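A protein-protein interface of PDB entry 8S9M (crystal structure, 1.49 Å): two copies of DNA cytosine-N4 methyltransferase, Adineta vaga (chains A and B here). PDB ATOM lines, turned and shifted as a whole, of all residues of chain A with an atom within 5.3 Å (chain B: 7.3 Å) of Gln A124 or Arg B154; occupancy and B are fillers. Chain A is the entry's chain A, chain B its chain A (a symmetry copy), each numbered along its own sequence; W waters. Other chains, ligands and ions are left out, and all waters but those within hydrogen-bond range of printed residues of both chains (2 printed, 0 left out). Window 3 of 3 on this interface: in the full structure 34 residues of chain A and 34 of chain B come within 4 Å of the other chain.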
ATOM      1  N   THR A 121     -20.979  -4.732 -20.094  1.00  0.00           N
ATOM      2  CA  THR A 121     -19.757  -5.518 -20.148  1.00  0.00           C
ATOM      3  C   THR A 121     -19.427  -5.833 -21.598  1.00  0.00           C
ATOM      4  O   THR A 121     -20.318  -5.974 -22.440  1.00  0.00           O
ATOM      5  CB  THR A 121     -19.901  -6.832 -19.355  1.00  0.00           C
ATOM      6  OG1 THR A 121     -18.739  -7.647 -19.551  1.00  0.00           O
ATOM      7  CG2 THR A 121     -21.137  -7.611 -19.794  1.00  0.00           C
ATOM      8  N   VAL A 122     -18.126  -5.942 -21.887  1.00  0.00           N
ATOM      9  CA  VAL A 122     -17.719  -6.376 -23.214  1.00  0.00           C
ATOM     10  C   VAL A 122     -18.018  -7.852 -23.435  1.00  0.00           C
ATOM     11  O   VAL A 122     -18.030  -8.314 -24.581  1.00  0.00           O
ATOM     12  CB  VAL A 122     -16.242  -6.041 -23.493  1.00  0.00           C
ATOM     13  CG1 VAL A 122     -16.017  -4.547 -23.406  1.00  0.00           C
ATOM     14  CG2 VAL A 122     -15.338  -6.778 -22.524  1.00  0.00           C
ATOM     15  N   ASN A 123     -18.272  -8.605 -22.367  1.00  0.00           N
ATOM     16  CA  ASN A 123     -18.513 -10.041 -22.479  1.00  0.00           C
ATOM     17  C   ASN A 123     -19.970 -10.268 -22.853  1.00  0.00           C
ATOM     18  O   ASN A 123     -20.858 -10.239 -21.995  1.00  0.00           O
ATOM     19  CB  ASN A 123     -18.168 -10.752 -21.177  1.00  0.00           C
ATOM     20  CG  ASN A 123     -18.391 -12.260 -21.259  1.00  0.00           C
ATOM     21  OD1 ASN A 123     -18.749 -12.794 -22.313  1.00  0.00           O
ATOM     22  ND2 ASN A 123     -18.165 -12.953 -20.150  1.00  0.00           N
ATOM     23  N   GLN A 124     -20.220 -10.537 -24.131  1.00  0.00           N
ATOM     24  CA  GLN A 124     -21.579 -10.732 -24.615  1.00  0.00           C
ATOM     25  C   GLN A 124     -21.925 -12.192 -24.884  1.00  0.00           C
ATOM     26  O   GLN A 124     -22.939 -12.467 -25.536  1.00  0.00           O
ATOM     27  CB  GLN A 124     -21.843  -9.856 -25.838  1.00  0.00           C
ATOM     28  CG  GLN A 124     -21.943  -8.384 -25.467  1.00  0.00           C
ATOM     29  CD  GLN A 124     -23.067  -8.127 -24.474  1.00  0.00           C
ATOM     30  OE1 GLN A 124     -24.194  -8.596 -24.664  1.00  0.00           O
ATOM     31  NE2 GLN A 124     -22.761  -7.403 -23.400  1.00  0.00           N
ATOM     32  N   ASN A 125     -21.114 -13.125 -24.386  1.00  0.00           N
ATOM     33  CA  ASN A 125     -21.408 -14.553 -24.480  1.00  0.00           C
ATOM     34  C   ASN A 125     -22.839 -14.826 -24.041  1.00  0.00           C
ATOM     35  O   ASN A 125     -23.204 -14.566 -22.892  1.00  0.00           O
ATOM     36  CB  ASN A 125     -20.426 -15.306 -23.576  1.00  0.00           C
ATOM     37  CG  ASN A 125     -20.464 -16.815 -23.771  1.00  0.00           C
ATOM     38  OD1 ASN A 125     -21.503 -17.395 -24.077  1.00  0.00           O
ATOM     39  ND2 ASN A 125     -19.318 -17.458 -23.578  1.00  0.00           N
ATOM     40  N   ALA A 126     -23.653 -15.351 -24.958  1.00  0.00           N
ATOM     41  CA  ALA A 126     -25.079 -15.530 -24.694  1.00  0.00           C
ATOM     42  C   ALA A 126     -25.398 -16.792 -23.902  1.00  0.00           C
ATOM     43  O   ALA A 126     -26.582 -17.099 -23.716  1.00  0.00           O
ATOM     44  CB  ALA A 126     -25.879 -15.500 -25.999  1.00  0.00           C
ATOM     45  N   TYR A 128     -24.997 -17.098 -20.779  1.00  0.00           N
ATOM     46  CA  TYR A 128     -25.397 -16.683 -19.439  1.00  0.00           C
ATOM     47  C   TYR A 128     -25.907 -15.252 -19.520  1.00  0.00           C
ATOM     48  O   TYR A 128     -25.900 -14.635 -20.587  1.00  0.00           O
ATOM     49  CB  TYR A 128     -24.254 -16.856 -18.428  1.00  0.00           C
ATOM     50  CG  TYR A 128     -22.883 -16.542 -18.974  1.00  0.00           C
ATOM     51  CD1 TYR A 128     -22.483 -15.232 -19.178  1.00  0.00           C
ATOM     52  CD2 TYR A 128     -21.976 -17.556 -19.257  1.00  0.00           C
ATOM     53  CE1 TYR A 128     -21.220 -14.934 -19.664  1.00  0.00           C
ATOM     54  CE2 TYR A 128     -20.713 -17.273 -19.742  1.00  0.00           C
ATOM     55  CZ  TYR A 128     -20.343 -15.957 -19.948  1.00  0.00           C
ATOM     56  OH  TYR A 128     -19.087 -15.656 -20.427  1.00  0.00           O
ATOM     57  N   PHE A 129     -26.379 -14.726 -18.389  1.00  0.00           N
ATOM     58  CA  PHE A 129     -26.793 -13.329 -18.364  1.00  0.00           C
ATOM     59  C   PHE A 129     -25.568 -12.412 -18.362  1.00  0.00           C
ATOM     60  O   PHE A 129     -24.511 -12.755 -17.833  1.00  0.00           O
ATOM     61  CB  PHE A 129     -27.690 -13.071 -17.152  1.00  0.00           C
ATOM     62  CG  PHE A 129     -29.020 -13.763 -17.253  1.00  0.00           C
ATOM     63  CD1 PHE A 129     -30.095 -13.142 -17.882  1.00  0.00           C
ATOM     64  CD2 PHE A 129     -29.183 -15.055 -16.766  1.00  0.00           C
ATOM     65  CE1 PHE A 129     -31.331 -13.797 -18.010  1.00  0.00           C
ATOM     66  CE2 PHE A 129     -30.411 -15.715 -16.885  1.00  0.00           C
ATOM     67  CZ  PHE A 129     -31.487 -15.085 -17.513  1.00  0.00           C
ATOM     68  N   ARG A 130     -25.720 -11.232 -18.961  1.00  0.00           N
ATOM     69  CA  ARG A 130     -24.574 -10.339 -19.167  1.00  0.00           C
ATOM     70  C   ARG A 130     -23.919  -9.997 -17.835  1.00  0.00           C
ATOM     71  O   ARG A 130     -24.591  -9.448 -16.945  1.00  0.00           O
ATOM     72  CB  ARG A 130     -25.003  -9.054 -19.851  1.00  0.00           C
ATOM     73  CG  ARG A 130     -25.495  -9.249 -21.270  1.00  0.00           C
ATOM     74  CD  ARG A 130     -26.116  -7.965 -21.768  1.00  0.00           C
ATOM     75  NE  ARG A 130     -26.493  -8.063 -23.172  1.00  0.00           N
ATOM     76  CZ  ARG A 130     -27.392  -7.282 -23.753  1.00  0.00           C
ATOM     77  NH1 ARG A 130     -28.044  -6.356 -23.071  1.00  0.00           N
ATOM     78  NH2 ARG A 130     -27.644  -7.437 -25.052  1.00  0.00           N
ATOM     79  N   PHE B 152     -30.316 -22.740 -22.685  1.00  0.00           N
ATOM     80  CA  PHE B 152     -30.529 -21.330 -22.358  1.00  0.00           C
ATOM     81  C   PHE B 152     -30.633 -20.533 -23.645  1.00  0.00           C
ATOM     82  O   PHE B 152     -29.702 -20.548 -24.458  1.00  0.00           O
ATOM     83  CB  PHE B 152     -29.376 -20.808 -21.503  1.00  0.00           C
ATOM     84  CG  PHE B 152     -29.531 -19.379 -21.078  1.00  0.00           C
ATOM     85  CD1 PHE B 152     -30.602 -18.985 -20.282  1.00  0.00           C
ATOM     86  CD2 PHE B 152     -28.586 -18.430 -21.447  1.00  0.00           C
ATOM     87  CE1 PHE B 152     -30.732 -17.663 -19.872  1.00  0.00           C
ATOM     88  CE2 PHE B 152     -28.704 -17.115 -21.028  1.00  0.00           C
ATOM     89  CZ  PHE B 152     -29.784 -16.729 -20.248  1.00  0.00           C
ATOM     90  N   HIS B 153     -31.738 -19.809 -23.809  1.00  0.00           N
ATOM     91  CA  HIS B 153     -32.032 -19.050 -25.025  1.00  0.00           C
ATOM     92  C   HIS B 153     -32.265 -17.593 -24.631  1.00  0.00           C
ATOM     93  O   HIS B 153     -33.404 -17.138 -24.528  1.00  0.00           O
ATOM     94  CB  HIS B 153     -33.262 -19.646 -25.711  1.00  0.00           C
ATOM     95  CG  HIS B 153     -33.112 -21.091 -26.070  1.00  0.00           C
ATOM     96  ND1 HIS B 153     -32.574 -21.504 -27.268  1.00  0.00           N
ATOM     97  CD2 HIS B 153     -33.416 -22.219 -25.384  1.00  0.00           C
ATOM     98  CE1 HIS B 153     -32.564 -22.825 -27.313  1.00  0.00           C
ATOM     99  NE2 HIS B 153     -33.070 -23.283 -26.182  1.00  0.00           N
ATOM    100  N   ARG B 154     -31.171 -16.856 -24.425  1.00  0.00           N
ATOM    101  CA  ARG B 154     -31.281 -15.464 -24.005  1.00  0.00           C
ATOM    102  C   ARG B 154     -31.953 -14.597 -25.063  1.00  0.00           C
ATOM    103  O   ARG B 154     -32.527 -13.552 -24.727  1.00  0.00           O
ATOM    104  CB  ARG B 154     -29.890 -14.918 -23.674  1.00  0.00           C
ATOM    105  CG  ARG B 154     -29.892 -13.708 -22.752  1.00  0.00           C
ATOM    106  CD  ARG B 154     -28.472 -13.282 -22.402  1.00  0.00           C
ATOM    107  NE  ARG B 154     -27.773 -12.654 -23.516  1.00  0.00           N
ATOM    108  CZ  ARG B 154     -26.516 -12.237 -23.456  1.00  0.00           C
ATOM    109  NH1 ARG B 154     -25.768 -12.453 -22.386  1.00  0.00           N
ATOM    110  NH2 ARG B 154     -25.999 -11.575 -24.492  1.00  0.00           N
ATOM    111  N   ASP B 155     -31.909 -15.025 -26.325  1.00  0.00           N
ATOM    112  CA  ASP B 155     -32.544 -14.300 -27.419  1.00  0.00           C
ATOM    113  C   ASP B 155     -34.047 -14.135 -27.229  1.00  0.00           C
ATOM    114  O   ASP B 155     -34.640 -13.255 -27.861  1.00  0.00           O
ATOM    115  CB  ASP B 155     -32.274 -15.038 -28.729  1.00  0.00           C
ATOM    116  CG  ASP B 155     -32.653 -16.513 -28.655  1.00  0.00           C
ATOM    117  OD1 ASP B 155     -31.942 -17.289 -27.980  1.00  0.00           O
ATOM    118  OD2 ASP B 155     -33.673 -16.893 -29.258  1.00  0.00           O
ATOM    119  N   ARG B 156     -34.674 -14.954 -26.383  1.00  0.00           N
ATOM    120  CA  ARG B 156     -36.109 -14.869 -26.147  1.00  0.00           C
ATOM    121  C   ARG B 156     -36.498 -13.721 -25.227  1.00  0.00           C
ATOM    122  O   ARG B 156     -37.692 -13.427 -25.101  1.00  0.00           O
ATOM    123  CB  ARG B 156     -36.623 -16.196 -25.578  1.00  0.00           C
ATOM    124  CG  ARG B 156     -36.376 -17.364 -26.513  1.00  0.00           C
ATOM    125  CD  ARG B 156     -36.770 -18.688 -25.886  1.00  0.00           C
ATOM    126  NE  ARG B 156     -36.538 -19.809 -26.792  1.00  0.00           N
ATOM    127  CZ  ARG B 156     -36.717 -21.083 -26.464  1.00  0.00           C
ATOM    128  NH1 ARG B 156     -37.103 -21.437 -25.247  1.00  0.00           N
ATOM    129  NH2 ARG B 156     -36.509 -22.025 -27.377  1.00  0.00           N
ATOM    130  N   LEU B 157     -35.512 -13.052 -24.582  1.00  0.00           N
ATOM    131  CA  LEU B 157     -35.818 -12.025 -23.598  1.00  0.00           C
ATOM    132  C   LEU B 157     -35.724 -10.637 -24.212  1.00  0.00           C
ATOM    133  O   LEU B 157     -34.936 -10.409 -25.133  1.00  0.00           O
ATOM    134  CB  LEU B 157     -34.803 -12.083 -22.456  1.00  0.00           C
ATOM    135  CG  LEU B 157     -34.823 -13.368 -21.643  1.00  0.00           C
ATOM    136  CD1 LEU B 157     -33.713 -13.342 -20.609  1.00  0.00           C
ATOM    137  CD2 LEU B 157     -36.185 -13.543 -20.992  1.00  0.00           C
ATOM    138  N   PRO B 158     -36.504  -9.692 -23.693  1.00  0.00           N
ATOM    139  CA  PRO B 158     -36.285  -8.291 -24.045  1.00  0.00           C
ATOM    140  C   PRO B 158     -34.945  -7.828 -23.498  1.00  0.00           C
ATOM    141  O   PRO B 158     -34.376  -8.427 -22.582  1.00  0.00           O
ATOM    142  CB  PRO B 158     -37.445  -7.562 -23.357  1.00  0.00           C
ATOM    143  CG  PRO B 158     -37.887  -8.467 -22.275  1.00  0.00           C
ATOM    144  CD  PRO B 158     -37.580  -9.865 -22.703  1.00  0.00           C
ATOM    145  N   GLU B 159     -34.448  -6.739 -24.087  1.00  0.00           N
ATOM    146  CA  GLU B 159     -33.121  -6.229 -23.758  1.00  0.00           C
ATOM    147  C   GLU B 159     -32.957  -6.012 -22.258  1.00  0.00           C
ATOM    148  O   GLU B 159     -31.899  -6.308 -21.692  1.00  0.00           O
ATOM    149  CB  GLU B 159     -32.893  -4.919 -24.514  1.00  0.00           C
ATOM    150  CG  GLU B 159     -31.529  -4.293 -24.323  1.00  0.00           C
ATOM    151  CD  GLU B 159     -30.450  -4.964 -25.147  1.00  0.00           C
ATOM    152  OE1 GLU B 159     -30.781  -5.832 -25.982  1.00  0.00           O
ATOM    153  OE2 GLU B 159     -29.265  -4.615 -24.959  1.00  0.00           O
ATOM    154  N   PHE B 161     -33.895  -7.558 -19.721  1.00  0.00           N
ATOM    155  CA  PHE B 161     -33.699  -8.726 -18.867  1.00  0.00           C
ATOM    156  C   PHE B 161     -32.551  -9.616 -19.323  1.00  0.00           C
ATOM    157  O   PHE B 161     -32.413 -10.733 -18.815  1.00  0.00           O
ATOM    158  CB  PHE B 161     -34.998  -9.531 -18.711  1.00  0.00           C
ATOM    159  CG  PHE B 161     -36.045  -8.835 -17.888  1.00  0.00           C
ATOM    160  CD1 PHE B 161     -35.737  -8.330 -16.629  1.00  0.00           C
ATOM    161  CD2 PHE B 161     -37.332  -8.669 -18.375  1.00  0.00           C
ATOM    162  CE1 PHE B 161     -36.702  -7.682 -15.870  1.00  0.00           C
ATOM    163  CE2 PHE B 161     -38.304  -8.028 -17.619  1.00  0.00           C
ATOM    164  CZ  PHE B 161     -37.987  -7.528 -16.369  1.00  0.00           C
ATOM    165  N   LYS B 162     -31.705  -9.145 -20.242  1.00  0.00           N
ATOM    166  CA  LYS B 162     -30.564  -9.935 -20.697  1.00  0.00           C
ATOM    167  C   LYS B 162     -29.371  -9.865 -19.750  1.00  0.00           C
ATOM    168  O   LYS B 162     -28.385 -10.584 -19.960  1.00  0.00           O
ATOM    169  CB  LYS B 162     -30.136  -9.486 -22.096  1.00  0.00           C
ATOM    170  CG  LYS B 162     -31.162  -9.777 -23.186  1.00  0.00           C
ATOM    171  CD  LYS B 162     -30.616  -9.319 -24.527  1.00  0.00           C
ATOM    172  CE  LYS B 162     -31.648  -9.454 -25.614  1.00  0.00           C
ATOM    173  NZ  LYS B 162     -31.898 -10.866 -25.970  1.00  0.00           N
ATOM    174  N   GLY B 163     -29.435  -9.022 -18.720  1.00  0.00           N
ATOM    175  CA  GLY B 163     -28.320  -8.815 -17.824  1.00  0.00           C
ATOM    176  C   GLY B 163     -28.504  -9.524 -16.489  1.00  0.00           C
ATOM    177  O   GLY B 163     -29.554 -10.074 -16.166  1.00  0.00           O
ATOM    178  N   LEU B 190     -39.030 -19.227 -19.746  1.00  0.00           N
ATOM    179  CA  LEU B 190     -38.960 -18.995 -21.186  1.00  0.00           C
ATOM    180  C   LEU B 190     -37.584 -19.335 -21.747  1.00  0.00           C
ATOM    181  O   LEU B 190     -37.475 -19.865 -22.858  1.00  0.00           O
ATOM    182  CB  LEU B 190     -39.317 -17.540 -21.487  1.00  0.00           C
ATOM    183  CG  LEU B 190     -39.293 -17.142 -22.960  1.00  0.00           C
ATOM    184  CD1 LEU B 190     -40.285 -17.986 -23.747  1.00  0.00           C
ATOM    185  CD2 LEU B 190     -39.599 -15.660 -23.115  1.00  0.00           C
ATOM    186  N   THR B 191     -36.523 -19.057 -20.991  1.00  0.00           N
ATOM    187  CA  THR B 191     -35.176 -19.222 -21.525  1.00  0.00           C
ATOM    188  C   THR B 191     -34.648 -20.648 -21.430  1.00  0.00           C
ATOM    189  O   THR B 191     -33.701 -20.983 -22.144  1.00  0.00           O
ATOM    190  CB  THR B 191     -34.194 -18.270 -20.834  1.00  0.00           C
ATOM    191  OG1 THR B 191     -34.150 -18.544 -19.425  1.00  0.00           O
ATOM    192  CG2 THR B 191     -34.602 -16.836 -21.061  1.00  0.00           C
ATOM    193  N   THR B 192     -35.216 -21.492 -20.571  1.00  0.00           N
ATOM    194  CA  THR B 192     -34.618 -22.792 -20.293  1.00  0.00           C
ATOM    195  C   THR B 192     -35.493 -23.971 -20.679  1.00  0.00           C
ATOM    196  O   THR B 192     -35.115 -25.116 -20.398  1.00  0.00           O
ATOM    197  CB  THR B 192     -34.232 -22.909 -18.811  1.00  0.00           C
ATOM    198  OG1 THR B 192     -35.415 -22.810 -18.004  1.00  0.00           O
ATOM    199  CG2 THR B 192     -33.234 -21.807 -18.414  1.00  0.00           C
HETATM  200  O   HOH W   1     -28.679 -17.991 -25.205  1.00  0.00           O
HETATM  201  O   HOH W   2     -22.998 -12.074 -21.750  1.00  0.00           O
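Among the printed residues, merely in contact across the chains: Ala A126 with Phe B152, Ala A126 with Arg B154, Tyr A128 with Phe B152, Phe A129 with Phe B152, Phe A129 with Leu B157, Phe A129 with Phe B161, Phe A129 with Lys B162, Phe A129 with Gly B163, Arg A130 with Arg B154 and Arg A130 with Gly B163.
The backbone carbonyl oxygen (O) of Thr A121 sits at hydrogen-bond distance from the side-chain amide nitrogen (NE2) of Gln A124 (3.0 Å). The side-chain amide oxygen (OD1) of Asn A123 is in hydrogen-bond range of the backbone NH (N) of Asn A125 (3.2 Å). ND2 of Asn A123 is in hydrogen-bond range of OH of Tyr A128 (2.9 Å). The guanidinium group of Arg A130 lies within hydrogen-bond range of the side-chain amide oxygen of Gln A124, at 2.8 Å. The side-chain amino group of Lys B162 is in hydrogen-bond range of the backbone carbonyl oxygen of Arg B154. The backbone carbonyl oxygen (O) of Leu B157 sits at hydrogen-bond distance from the side-chain amino group (NZ) of Lys B162, at 3.2 Å.
No position is printed for both chains. Of the 15 pairs that touch across the chains among the printed residues, none has its exchanged pair printed and touching as well.
O of Gln A124 lies within hydrogen-bond range of NH2 of Arg B154 (3.4 Å). The backbone carbonyl oxygen of Asn A125 lies within hydrogen-bond range of the guanidinium group of Arg B154. NH1 of Arg B154 lies within hydrogen-bond range of O of Tyr A128 (2.8 Å). The guanidinium group of Arg A130 lies within salt-bridge range of the side-chain carboxylate of Glu B159 (2.8 Å). The backbone carbonyl oxygen (O) of Lys B162 sits at hydrogen-bond distance from the backbone NH (N) of Arg A130.
Of the 14 printed residues of chain B, 7 touch a printed residue of chain A. Printed residues of chain B that touch a printed residue of chain A: Phe B152, Arg B154, Leu B157, Glu B159, Phe B161, Lys B162 and Gly B163. Hydrophobic or aromatic side chains of chain B within 4 Å of the printed part of chain A: Phe B152 and Leu B157. Of the 9 printed residues of chain A, 6 touch a printed residue of chain B. Among the printed residues, Asp or Glu carboxylates within 4 Å of a Lys or Arg side-chain nitrogen of the other chain: Arg A130 with Glu B159.
Gln A124 touches one residue of chain B. Printed residues of chain B within 4 Å of Arg A130: Arg B154, Glu B159, Lys B162 and Gly B163. Printed residues of chain B within 4 Å of Phe A129: Phe B152 (3.6 Å), Leu B157 (3.6 Å), Phe B161 (3.3 Å), Lys B162 (3.6 Å) and Gly B163 (3.6 Å). Thr B192 touches none of the printed residues of chain A. His B153 touches none of the printed residues of chain A. The nearest residue of chain A that does not touch Arg B154 is Phe A129 (4.03 Å).
Water W1 lies within hydrogen-bond range of the backbone carbonyl oxygen of Ala A126, the backbone NH of Arg B154 and the backbone carbonyl oxygen of Phe B152. Water W2 lies within hydrogen-bond range of the backbone carbonyl oxygen (O) of Asn A125 (2.7 Å), the backbone carbonyl oxygen (O) of Asn A123 (2.8 Å) and the guanidinium group (NH1) of Arg B154 (2.9 Å).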
